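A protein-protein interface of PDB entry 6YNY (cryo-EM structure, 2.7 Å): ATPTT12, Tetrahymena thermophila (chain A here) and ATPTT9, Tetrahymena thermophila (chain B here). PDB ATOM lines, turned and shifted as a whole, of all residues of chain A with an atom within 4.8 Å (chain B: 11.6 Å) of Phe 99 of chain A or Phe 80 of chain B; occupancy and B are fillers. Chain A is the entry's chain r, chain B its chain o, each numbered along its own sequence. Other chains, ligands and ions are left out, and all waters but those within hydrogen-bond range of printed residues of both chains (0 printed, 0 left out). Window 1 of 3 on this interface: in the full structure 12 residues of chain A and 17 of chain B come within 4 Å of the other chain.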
ATOM      1  N   TYR A  95       8.897 -35.934 -23.806  1.00  0.00           N
ATOM      2  CA  TYR A  95       8.035 -34.759 -23.774  1.00  0.00           C
ATOM      3  C   TYR A  95       6.579 -35.158 -23.585  1.00  0.00           C
ATOM      4  O   TYR A  95       5.855 -34.539 -22.800  1.00  0.00           O
ATOM      5  CB  TYR A  95       8.206 -33.956 -25.061  1.00  0.00           C
ATOM      6  CG  TYR A  95       7.166 -32.881 -25.267  1.00  0.00           C
ATOM      7  CD1 TYR A  95       7.393 -31.580 -24.857  1.00  0.00           C
ATOM      8  CD2 TYR A  95       5.957 -33.167 -25.876  1.00  0.00           C
ATOM      9  CE1 TYR A  95       6.449 -30.603 -25.045  1.00  0.00           C
ATOM     10  CE2 TYR A  95       5.009 -32.200 -26.063  1.00  0.00           C
ATOM     11  CZ  TYR A  95       5.257 -30.917 -25.650  1.00  0.00           C
ATOM     12  OH  TYR A  95       4.310 -29.946 -25.839  1.00  0.00           O
ATOM     13  N   ASN A  96       6.135 -36.191 -24.301  1.00  0.00           N
ATOM     14  CA  ASN A  96       4.754 -36.636 -24.186  1.00  0.00           C
ATOM     15  C   ASN A  96       4.468 -37.199 -22.802  1.00  0.00           C
ATOM     16  O   ASN A  96       3.390 -36.969 -22.243  1.00  0.00           O
ATOM     17  CB  ASN A  96       4.453 -37.673 -25.261  1.00  0.00           C
ATOM     18  CG  ASN A  96       4.538 -37.104 -26.653  1.00  0.00           C
ATOM     19  OD1 ASN A  96       4.487 -35.893 -26.846  1.00  0.00           O
ATOM     20  ND2 ASN A  96       4.659 -37.977 -27.633  1.00  0.00           N
ATOM     21  N   ARG A  97       5.418 -37.941 -22.234  1.00  0.00           N
ATOM     22  CA  ARG A  97       5.247 -38.441 -20.876  1.00  0.00           C
ATOM     23  C   ARG A  97       5.047 -37.296 -19.895  1.00  0.00           C
ATOM     24  O   ARG A  97       4.128 -37.322 -19.069  1.00  0.00           O
ATOM     25  CB  ARG A  97       6.452 -39.284 -20.473  1.00  0.00           C
ATOM     26  CG  ARG A  97       6.475 -40.676 -21.056  1.00  0.00           C
ATOM     27  CD  ARG A  97       5.320 -41.502 -20.554  1.00  0.00           C
ATOM     28  NE  ARG A  97       5.492 -42.919 -20.836  1.00  0.00           N
ATOM     29  CZ  ARG A  97       4.544 -43.832 -20.669  1.00  0.00           C
ATOM     30  NH1 ARG A  97       3.346 -43.482 -20.230  1.00  0.00           N
ATOM     31  NH2 ARG A  97       4.791 -45.101 -20.947  1.00  0.00           N
ATOM     32  N   GLN A  98       5.902 -36.279 -19.968  1.00  0.00           N
ATOM     33  CA  GLN A  98       5.744 -35.129 -19.091  1.00  0.00           C
ATOM     34  C   GLN A  98       4.478 -34.353 -19.420  1.00  0.00           C
ATOM     35  O   GLN A  98       3.905 -33.701 -18.543  1.00  0.00           O
ATOM     36  CB  GLN A  98       6.970 -34.228 -19.189  1.00  0.00           C
ATOM     37  CG  GLN A  98       7.015 -33.130 -18.158  1.00  0.00           C
ATOM     38  CD  GLN A  98       7.106 -33.652 -16.750  1.00  0.00           C
ATOM     39  OE1 GLN A  98       7.452 -34.808 -16.523  1.00  0.00           O
ATOM     40  NE2 GLN A  98       6.791 -32.800 -15.790  1.00  0.00           N
ATOM     41  N   PHE A  99       4.035 -34.407 -20.675  1.00  0.00           N
ATOM     42  CA  PHE A  99       2.752 -33.818 -21.029  1.00  0.00           C
ATOM     43  C   PHE A  99       1.604 -34.559 -20.361  1.00  0.00           C
ATOM     44  O   PHE A  99       0.589 -33.947 -20.018  1.00  0.00           O
ATOM     45  CB  PHE A  99       2.578 -33.824 -22.545  1.00  0.00           C
ATOM     46  CG  PHE A  99       1.491 -32.924 -23.030  1.00  0.00           C
ATOM     47  CD1 PHE A  99       1.783 -31.657 -23.482  1.00  0.00           C
ATOM     48  CD2 PHE A  99       0.176 -33.340 -23.030  1.00  0.00           C
ATOM     49  CE1 PHE A  99       0.791 -30.824 -23.925  1.00  0.00           C
ATOM     50  CE2 PHE A  99      -0.819 -32.509 -23.471  1.00  0.00           C
ATOM     51  CZ  PHE A  99      -0.511 -31.249 -23.920  1.00  0.00           C
ATOM     52  N   GLN A 100       1.746 -35.871 -20.172  1.00  0.00           N
ATOM     53  CA  GLN A 100       0.736 -36.636 -19.454  1.00  0.00           C
ATOM     54  C   GLN A 100       0.737 -36.291 -17.972  1.00  0.00           C
ATOM     55  O   GLN A 100      -0.323 -36.088 -17.371  1.00  0.00           O
ATOM     56  CB  GLN A 100       0.980 -38.128 -19.650  1.00  0.00           C
ATOM     57  CG  GLN A 100       0.822 -38.611 -21.063  1.00  0.00           C
ATOM     58  CD  GLN A 100       1.270 -40.039 -21.232  1.00  0.00           C
ATOM     59  OE1 GLN A 100       2.231 -40.478 -20.606  1.00  0.00           O
ATOM     60  NE2 GLN A 100       0.567 -40.781 -22.070  1.00  0.00           N
ATOM     61  N   ARG A 101       1.923 -36.228 -17.364  1.00  0.00           N
ATOM     62  CA  ARG A 101       2.009 -35.850 -15.959  1.00  0.00           C
ATOM     63  C   ARG A 101       1.464 -34.451 -15.727  1.00  0.00           C
ATOM     64  O   ARG A 101       0.871 -34.181 -14.678  1.00  0.00           O
ATOM     65  CB  ARG A 101       3.456 -35.934 -15.481  1.00  0.00           C
ATOM     66  CG  ARG A 101       4.115 -37.264 -15.733  1.00  0.00           C
ATOM     67  CD  ARG A 101       5.485 -37.341 -15.105  1.00  0.00           C
ATOM     68  NE  ARG A 101       6.242 -38.493 -15.587  1.00  0.00           N
ATOM     69  CZ  ARG A 101       7.155 -38.455 -16.552  1.00  0.00           C
ATOM     70  NH1 ARG A 101       7.455 -37.317 -17.157  1.00  0.00           N
ATOM     71  NH2 ARG A 101       7.777 -39.566 -16.913  1.00  0.00           N
ATOM     72  N   MET A 102       1.648 -33.553 -16.693  1.00  0.00           N
ATOM     73  CA  MET A 102       1.149 -32.192 -16.546  1.00  0.00           C
ATOM     74  C   MET A 102      -0.372 -32.155 -16.572  1.00  0.00           C
ATOM     75  O   MET A 102      -0.992 -31.416 -15.801  1.00  0.00           O
ATOM     76  CB  MET A 102       1.738 -31.313 -17.647  1.00  0.00           C
ATOM     77  CG  MET A 102       1.262 -29.873 -17.640  1.00  0.00           C
ATOM     78  SD  MET A 102      -0.262 -29.607 -18.554  1.00  0.00           S
ATOM     79  CE  MET A 102       0.309 -29.913 -20.216  1.00  0.00           C
ATOM     80  N   ARG A 103      -0.993 -32.945 -17.451  1.00  0.00           N
ATOM     81  CA  ARG A 103      -2.449 -32.975 -17.505  1.00  0.00           C
ATOM     82  C   ARG A 103      -3.037 -33.724 -16.321  1.00  0.00           C
ATOM     83  O   ARG A 103      -4.159 -33.425 -15.900  1.00  0.00           O
ATOM     84  CB  ARG A 103      -2.918 -33.594 -18.819  1.00  0.00           C
ATOM     85  CG  ARG A 103      -2.676 -32.735 -20.042  1.00  0.00           C
ATOM     86  CD  ARG A 103      -3.243 -31.343 -19.875  1.00  0.00           C
ATOM     87  NE  ARG A 103      -3.264 -30.580 -21.114  1.00  0.00           N
ATOM     88  CZ  ARG A 103      -3.320 -29.254 -21.167  1.00  0.00           C
ATOM     89  NH1 ARG A 103      -3.348 -28.542 -20.054  1.00  0.00           N
ATOM     90  NH2 ARG A 103      -3.338 -28.635 -22.335  1.00  0.00           N
ATOM     91  N   ASN B  60      -7.428 -23.144 -16.860  1.00  0.00           N
ATOM     92  CA  ASN B  60      -6.843 -24.340 -16.281  1.00  0.00           C
ATOM     93  C   ASN B  60      -5.783 -23.931 -15.273  1.00  0.00           C
ATOM     94  O   ASN B  60      -5.079 -22.938 -15.470  1.00  0.00           O
ATOM     95  CB  ASN B  60      -6.221 -25.240 -17.355  1.00  0.00           C
ATOM     96  CG  ASN B  60      -7.222 -25.696 -18.386  1.00  0.00           C
ATOM     97  OD1 ASN B  60      -6.979 -25.597 -19.586  1.00  0.00           O
ATOM     98  ND2 ASN B  60      -8.357 -26.199 -17.927  1.00  0.00           N
ATOM     99  N   ILE B  61      -5.682 -24.697 -14.193  1.00  0.00           N
ATOM    100  CA  ILE B  61      -4.661 -24.500 -13.174  1.00  0.00           C
ATOM    101  C   ILE B  61      -3.684 -25.659 -13.284  1.00  0.00           C
ATOM    102  O   ILE B  61      -4.071 -26.823 -13.128  1.00  0.00           O
ATOM    103  CB  ILE B  61      -5.263 -24.430 -11.763  1.00  0.00           C
ATOM    104  CG1 ILE B  61      -6.363 -23.372 -11.679  1.00  0.00           C
ATOM    105  CG2 ILE B  61      -4.189 -24.116 -10.760  1.00  0.00           C
ATOM    106  CD1 ILE B  61      -5.874 -21.975 -11.714  1.00  0.00           C
ATOM    107  N   VAL B  62      -2.424 -25.345 -13.559  1.00  0.00           N
ATOM    108  CA  VAL B  62      -1.376 -26.342 -13.722  1.00  0.00           C
ATOM    109  C   VAL B  62      -0.422 -26.240 -12.544  1.00  0.00           C
ATOM    110  O   VAL B  62      -0.131 -25.141 -12.060  1.00  0.00           O
ATOM    111  CB  VAL B  62      -0.623 -26.166 -15.054  1.00  0.00           C
ATOM    112  CG1 VAL B  62       0.370 -27.281 -15.242  1.00  0.00           C
ATOM    113  CG2 VAL B  62      -1.599 -26.144 -16.210  1.00  0.00           C
ATOM    114  N   HIS B  63       0.060 -27.391 -12.080  1.00  0.00           N
ATOM    115  CA  HIS B  63       0.903 -27.449 -10.898  1.00  0.00           C
ATOM    116  C   HIS B  63       2.380 -27.604 -11.222  1.00  0.00           C
ATOM    117  O   HIS B  63       3.211 -27.442 -10.323  1.00  0.00           O
ATOM    118  CB  HIS B  63       0.460 -28.603  -9.999  1.00  0.00           C
ATOM    119  CG  HIS B  63      -0.825 -28.345  -9.277  1.00  0.00           C
ATOM    120  ND1 HIS B  63      -1.144 -27.117  -8.742  1.00  0.00           N
ATOM    121  CD2 HIS B  63      -1.875 -29.156  -9.011  1.00  0.00           C
ATOM    122  CE1 HIS B  63      -2.333 -27.184  -8.172  1.00  0.00           C
ATOM    123  NE2 HIS B  63      -2.798 -28.411  -8.321  1.00  0.00           N
ATOM    124  N   VAL B  64       2.727 -27.929 -12.463  1.00  0.00           N
ATOM    125  CA  VAL B  64       4.123 -28.078 -12.862  1.00  0.00           C
ATOM    126  C   VAL B  64       4.462 -26.996 -13.880  1.00  0.00           C
ATOM    127  O   VAL B  64       3.576 -26.539 -14.615  1.00  0.00           O
ATOM    128  CB  VAL B  64       4.410 -29.479 -13.422  1.00  0.00           C
ATOM    129  CG1 VAL B  64       4.301 -30.505 -12.323  1.00  0.00           C
ATOM    130  CG2 VAL B  64       3.479 -29.811 -14.573  1.00  0.00           C
ATOM    131  N   PRO B  65       5.717 -26.558 -13.960  1.00  0.00           N
ATOM    132  CA  PRO B  65       6.064 -25.497 -14.907  1.00  0.00           C
ATOM    133  C   PRO B  65       5.850 -25.924 -16.351  1.00  0.00           C
ATOM    134  O   PRO B  65       6.015 -27.091 -16.710  1.00  0.00           O
ATOM    135  CB  PRO B  65       7.546 -25.238 -14.621  1.00  0.00           C
ATOM    136  CG  PRO B  65       7.779 -25.777 -13.276  1.00  0.00           C
ATOM    137  CD  PRO B  65       6.870 -26.943 -13.135  1.00  0.00           C
ATOM    138  N   VAL B  66       5.485 -24.951 -17.182  1.00  0.00           N
ATOM    139  CA  VAL B  66       5.371 -25.143 -18.619  1.00  0.00           C
ATOM    140  C   VAL B  66       5.860 -23.880 -19.308  1.00  0.00           C
ATOM    141  O   VAL B  66       5.746 -22.774 -18.771  1.00  0.00           O
ATOM    142  CB  VAL B  66       3.926 -25.462 -19.064  1.00  0.00           C
ATOM    143  CG1 VAL B  66       3.403 -26.684 -18.359  1.00  0.00           C
ATOM    144  CG2 VAL B  66       3.024 -24.284 -18.809  1.00  0.00           C
ATOM    145  N   HIS B  67       6.413 -24.051 -20.503  1.00  0.00           N
ATOM    146  CA  HIS B  67       6.867 -22.940 -21.324  1.00  0.00           C
ATOM    147  C   HIS B  67       6.053 -22.902 -22.607  1.00  0.00           C
ATOM    148  O   HIS B  67       5.960 -23.908 -23.318  1.00  0.00           O
ATOM    149  CB  HIS B  67       8.354 -23.056 -21.644  1.00  0.00           C
ATOM    150  CG  HIS B  67       8.929 -21.827 -22.271  1.00  0.00           C
ATOM    151  ND1 HIS B  67       9.355 -21.789 -23.580  1.00  0.00           N
ATOM    152  CD2 HIS B  67       9.135 -20.586 -21.772  1.00  0.00           C
ATOM    153  CE1 HIS B  67       9.807 -20.580 -23.859  1.00  0.00           C
ATOM    154  NE2 HIS B  67       9.683 -19.831 -22.778  1.00  0.00           N
ATOM    155  N   MET B  68       5.468 -21.747 -22.896  1.00  0.00           N
ATOM    156  CA  MET B  68       4.625 -21.561 -24.064  1.00  0.00           C
ATOM    157  C   MET B  68       5.417 -20.937 -25.202  1.00  0.00           C
ATOM    158  O   MET B  68       6.314 -20.120 -24.986  1.00  0.00           O
ATOM    159  CB  MET B  68       3.424 -20.679 -23.729  1.00  0.00           C
ATOM    160  CG  MET B  68       2.340 -21.373 -22.931  1.00  0.00           C
ATOM    161  SD  MET B  68       1.409 -22.548 -23.925  1.00  0.00           S
ATOM    162  CE  MET B  68       0.076 -22.933 -22.804  1.00  0.00           C
ATOM    163  N   GLY B  69       5.076 -21.335 -26.425  1.00  0.00           N
ATOM    164  CA  GLY B  69       5.750 -20.801 -27.591  1.00  0.00           C
ATOM    165  C   GLY B  69       5.264 -19.400 -27.916  1.00  0.00           C
ATOM    166  O   GLY B  69       4.069 -19.109 -27.897  1.00  0.00           O
ATOM    167  N   ASP B  75      -0.444 -21.279 -30.503  1.00  0.00           N
ATOM    168  CA  ASP B  75      -0.361 -21.221 -29.045  1.00  0.00           C
ATOM    169  C   ASP B  75      -0.231 -22.645 -28.530  1.00  0.00           C
ATOM    170  O   ASP B  75      -1.173 -23.434 -28.645  1.00  0.00           O
ATOM    171  CB  ASP B  75      -1.592 -20.541 -28.450  1.00  0.00           C
ATOM    172  CG  ASP B  75      -1.541 -20.457 -26.943  1.00  0.00           C
ATOM    173  OD1 ASP B  75      -0.442 -20.620 -26.374  1.00  0.00           O
ATOM    174  OD2 ASP B  75      -2.604 -20.241 -26.325  1.00  0.00           O
ATOM    175  N   TYR B  76       0.923 -22.973 -27.959  1.00  0.00           N
ATOM    176  CA  TYR B  76       1.175 -24.335 -27.517  1.00  0.00           C
ATOM    177  C   TYR B  76       2.331 -24.342 -26.530  1.00  0.00           C
ATOM    178  O   TYR B  76       2.999 -23.331 -26.312  1.00  0.00           O
ATOM    179  CB  TYR B  76       1.478 -25.254 -28.699  1.00  0.00           C
ATOM    180  CG  TYR B  76       2.766 -24.926 -29.409  1.00  0.00           C
ATOM    181  CD1 TYR B  76       3.923 -25.631 -29.142  1.00  0.00           C
ATOM    182  CD2 TYR B  76       2.826 -23.909 -30.343  1.00  0.00           C
ATOM    183  CE1 TYR B  76       5.097 -25.338 -29.784  1.00  0.00           C
ATOM    184  CE2 TYR B  76       3.996 -23.610 -30.990  1.00  0.00           C
ATOM    185  CZ  TYR B  76       5.130 -24.326 -30.707  1.00  0.00           C
ATOM    186  OH  TYR B  76       6.303 -24.029 -31.352  1.00  0.00           O
ATOM    187  N   ILE B  77       2.557 -25.511 -25.945  1.00  0.00           N
ATOM    188  CA  ILE B  77       3.639 -25.737 -24.997  1.00  0.00           C
ATOM    189  C   ILE B  77       4.800 -26.342 -25.768  1.00  0.00           C
ATOM    190  O   ILE B  77       4.723 -27.484 -26.233  1.00  0.00           O
ATOM    191  CB  ILE B  77       3.195 -26.647 -23.846  1.00  0.00           C
ATOM    192  CG1 ILE B  77       2.100 -25.962 -23.031  1.00  0.00           C
ATOM    193  CG2 ILE B  77       4.371 -26.998 -22.970  1.00  0.00           C
ATOM    194  CD1 ILE B  77       1.372 -26.877 -22.099  1.00  0.00           C
ATOM    195  N   ASP B  78       5.880 -25.581 -25.906  1.00  0.00           N
ATOM    196  CA  ASP B  78       7.020 -26.016 -26.699  1.00  0.00           C
ATOM    197  C   ASP B  78       8.061 -26.773 -25.892  1.00  0.00           C
ATOM    198  O   ASP B  78       8.853 -27.518 -26.478  1.00  0.00           O
ATOM    199  CB  ASP B  78       7.683 -24.813 -27.373  1.00  0.00           C
ATOM    200  CG  ASP B  78       8.184 -23.791 -26.379  1.00  0.00           C
ATOM    201  OD1 ASP B  78       7.570 -23.659 -25.301  1.00  0.00           O
ATOM    202  OD2 ASP B  78       9.190 -23.115 -26.676  1.00  0.00           O
ATOM    203  N   SER B  79       8.085 -26.610 -24.572  1.00  0.00           N
ATOM    204  CA  SER B  79       9.120 -27.234 -23.767  1.00  0.00           C
ATOM    205  C   SER B  79       8.671 -27.295 -22.318  1.00  0.00           C
ATOM    206  O   SER B  79       7.782 -26.557 -21.890  1.00  0.00           O
ATOM    207  CB  SER B  79      10.438 -26.466 -23.876  1.00  0.00           C
ATOM    208  OG  SER B  79      10.280 -25.130 -23.439  1.00  0.00           O
ATOM    209  N   PHE B  80       9.302 -28.197 -21.570  1.00  0.00           N
ATOM    210  CA  PHE B  80       9.125 -28.294 -20.138  1.00  0.00           C
ATOM    211  C   PHE B  80      10.445 -27.984 -19.446  1.00  0.00           C
ATOM    212  O   PHE B  80      11.466 -28.608 -19.769  1.00  0.00           O
ATOM    213  CB  PHE B  80       8.641 -29.689 -19.735  1.00  0.00           C
ATOM    214  CG  PHE B  80       7.243 -29.988 -20.170  1.00  0.00           C
ATOM    215  CD1 PHE B  80       6.167 -29.450 -19.496  1.00  0.00           C
ATOM    216  CD2 PHE B  80       7.003 -30.808 -21.250  1.00  0.00           C
ATOM    217  CE1 PHE B  80       4.886 -29.722 -19.893  1.00  0.00           C
ATOM    218  CE2 PHE B  80       5.722 -31.082 -21.648  1.00  0.00           C
ATOM    219  CZ  PHE B  80       4.662 -30.538 -20.969  1.00  0.00           C
ATOM    220  N   PRO B  81      10.479 -27.039 -18.509  1.00  0.00           N
ATOM    221  CA  PRO B  81      11.752 -26.686 -17.871  1.00  0.00           C
ATOM    222  C   PRO B  81      12.400 -27.878 -17.181  1.00  0.00           C
ATOM    223  O   PRO B  81      11.744 -28.644 -16.473  1.00  0.00           O
ATOM    224  CB  PRO B  81      11.352 -25.600 -16.868  1.00  0.00           C
ATOM    225  CG  PRO B  81      10.113 -25.028 -17.413  1.00  0.00           C
ATOM    226  CD  PRO B  81       9.394 -26.140 -18.086  1.00  0.00           C
ATOM    227  N   LYS B  82      13.706 -28.027 -17.399  1.00  0.00           N
ATOM    228  CA  LYS B  82      14.512 -29.053 -16.742  1.00  0.00           C
ATOM    229  C   LYS B  82      13.982 -30.454 -17.041  1.00  0.00           C
ATOM    230  O   LYS B  82      13.808 -31.284 -16.148  1.00  0.00           O
ATOM    231  CB  LYS B  82      14.585 -28.803 -15.235  1.00  0.00           C
ATOM    232  CG  LYS B  82      15.247 -27.486 -14.873  1.00  0.00           C
ATOM    233  CD  LYS B  82      15.536 -27.383 -13.388  1.00  0.00           C
ATOM    234  CE  LYS B  82      14.260 -27.356 -12.569  1.00  0.00           C
ATOM    235  NZ  LYS B  82      14.537 -27.159 -11.116  1.00  0.00           N
ATOM    236  N   LEU B  83      13.726 -30.713 -18.317  1.00  0.00           N
ATOM    237  CA  LEU B  83      13.285 -32.025 -18.765  1.00  0.00           C
ATOM    238  C   LEU B  83      14.501 -32.867 -19.126  1.00  0.00           C
ATOM    239  O   LEU B  83      15.273 -32.501 -20.019  1.00  0.00           O
ATOM    240  CB  LEU B  83      12.344 -31.904 -19.960  1.00  0.00           C
ATOM    241  CG  LEU B  83      11.786 -33.227 -20.474  1.00  0.00           C
ATOM    242  CD1 LEU B  83      10.971 -33.901 -19.400  1.00  0.00           C
ATOM    243  CD2 LEU B  83      10.948 -33.010 -21.705  1.00  0.00           C
ATOM    244  N   LYS B  84      14.672 -33.986 -18.432  1.00  0.00           N
ATOM    245  CA  LYS B  84      15.763 -34.914 -18.691  1.00  0.00           C
ATOM    246  C   LYS B  84      15.251 -36.068 -19.538  1.00  0.00           C
ATOM    247  O   LYS B  84      14.197 -36.642 -19.244  1.00  0.00           O
ATOM    248  CB  LYS B  84      16.361 -35.437 -17.386  1.00  0.00           C
ATOM    249  CG  LYS B  84      17.526 -34.610 -16.868  1.00  0.00           C
ATOM    250  CD  LYS B  84      17.123 -33.164 -16.636  1.00  0.00           C
ATOM    251  CE  LYS B  84      18.296 -32.327 -16.170  1.00  0.00           C
ATOM    252  NZ  LYS B  84      17.912 -30.903 -15.967  1.00  0.00           N
ATOM    253  N   GLU B  85      15.993 -36.400 -20.589  1.00  0.00           N
ATOM    254  CA  GLU B  85      15.641 -37.504 -21.472  1.00  0.00           C
ATOM    255  C   GLU B  85      16.245 -38.784 -20.911  1.00  0.00           C
ATOM    256  O   GLU B  85      17.469 -38.932 -20.858  1.00  0.00           O
ATOM    257  CB  GLU B  85      16.144 -37.249 -22.889  1.00  0.00           C
ATOM    258  CG  GLU B  85      15.691 -35.939 -23.485  1.00  0.00           C
ATOM    259  CD  GLU B  85      16.228 -35.726 -24.881  1.00  0.00           C
ATOM    260  OE1 GLU B  85      16.673 -36.714 -25.504  1.00  0.00           O
ATOM    261  OE2 GLU B  85      16.214 -34.572 -25.356  1.00  0.00           O
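No residue of chain B comes within 4 Å of Asn 96 of chain A.
Of the printed residues of chain B, Gln 98 of chain A touches Phe 80.
No residue of chain B comes within 4 Å of Arg 101 of chain A.
Met 102 of chain A touches just these residues of chain B: Val 62, Val 64, Val 66 and Ile 77.
No residue of chain B comes within 4 Å of Arg 103 of chain A.
Printed residues of chain A within 4 Å of Val 64 of chain B: Met 102 (3.8 Å).
Pro 65 of chain B touches none of the printed residues of chain A.
Of the printed residues of chain A, Ile 77 of chain B touches Tyr 95 (2.5 Å) and Met 102 (3.7 Å).
Of chain A, only Tyr 95 (3.5 Å), Gln 98 (3.7 Å) and Phe 99 (3.8 Å) come within 4 Å of Phe 80 of chain B.
The nearest residue of chain B that does not touch Phe 99 of chain A is Ile 77 of chain B (4.4 Å).
The backbone carbonyl oxygen (O) of Ile 77 of chain B is in hydrogen-bond range of the side-chain hydroxyl (OH) of Tyr 95 of chain A (2.5 Å).
Of the 9 printed residues of chain A, 4 touch a printed residue of chain B.
Printed residues of chain A that touch a printed residue of chain B: Tyr 95, Gln 98, Phe 99 and Met 102.
Hydrophobic or aromatic side chains of chain A within 4 Å of the printed part of chain B: Tyr 95, Phe 99 and Met 102.
Hydrophobic or aromatic side chains of chain B within 4 Å of the printed part of chain A: Val 62, Val 64, Val 66, Ile 77, Phe 80 and Leu 83.
Among the printed residues, no Asp or Glu carboxylate lies within 4 Å of a Lys or Arg side-chain nitrogen of the other chain.
Among the printed residues, pairs that only touch across the chains: Tyr 95 of chain A with Phe 80 of chain B (3.5 Å), Met 102 of chain A with Val 62 of chain B (3.6 Å), Met 102 of chain A with Ile 77 of chain B (3.7 Å), Gln 98 of chain A with Phe 80 of chain B (3.7 Å), Met 102 of chain A with Val 64 of chain B (3.8 Å), Phe 99 of chain A with Phe 80 of chain B (3.8 Å), Met 102 of chain A with Val 66 of chain B (3.9 Å) and Tyr 95 of chain A with Leu 83 of chain B (3.98 Å).
The guanidinium group (NH1) of Arg 101 of chain A lies within hydrogen-bond range of the side-chain amide oxygen (OE1) of Gln 98 of chain A (2.6 Å).
The backbone NH (N) of Ile 77 of chain B sits close to the side-chain sulfur (SD) of Met 68 of chain B.
SD of Met 102 of chain A sits at hydrogen-bond distance from NH1 of Arg 103 of chain A (3.6 Å).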
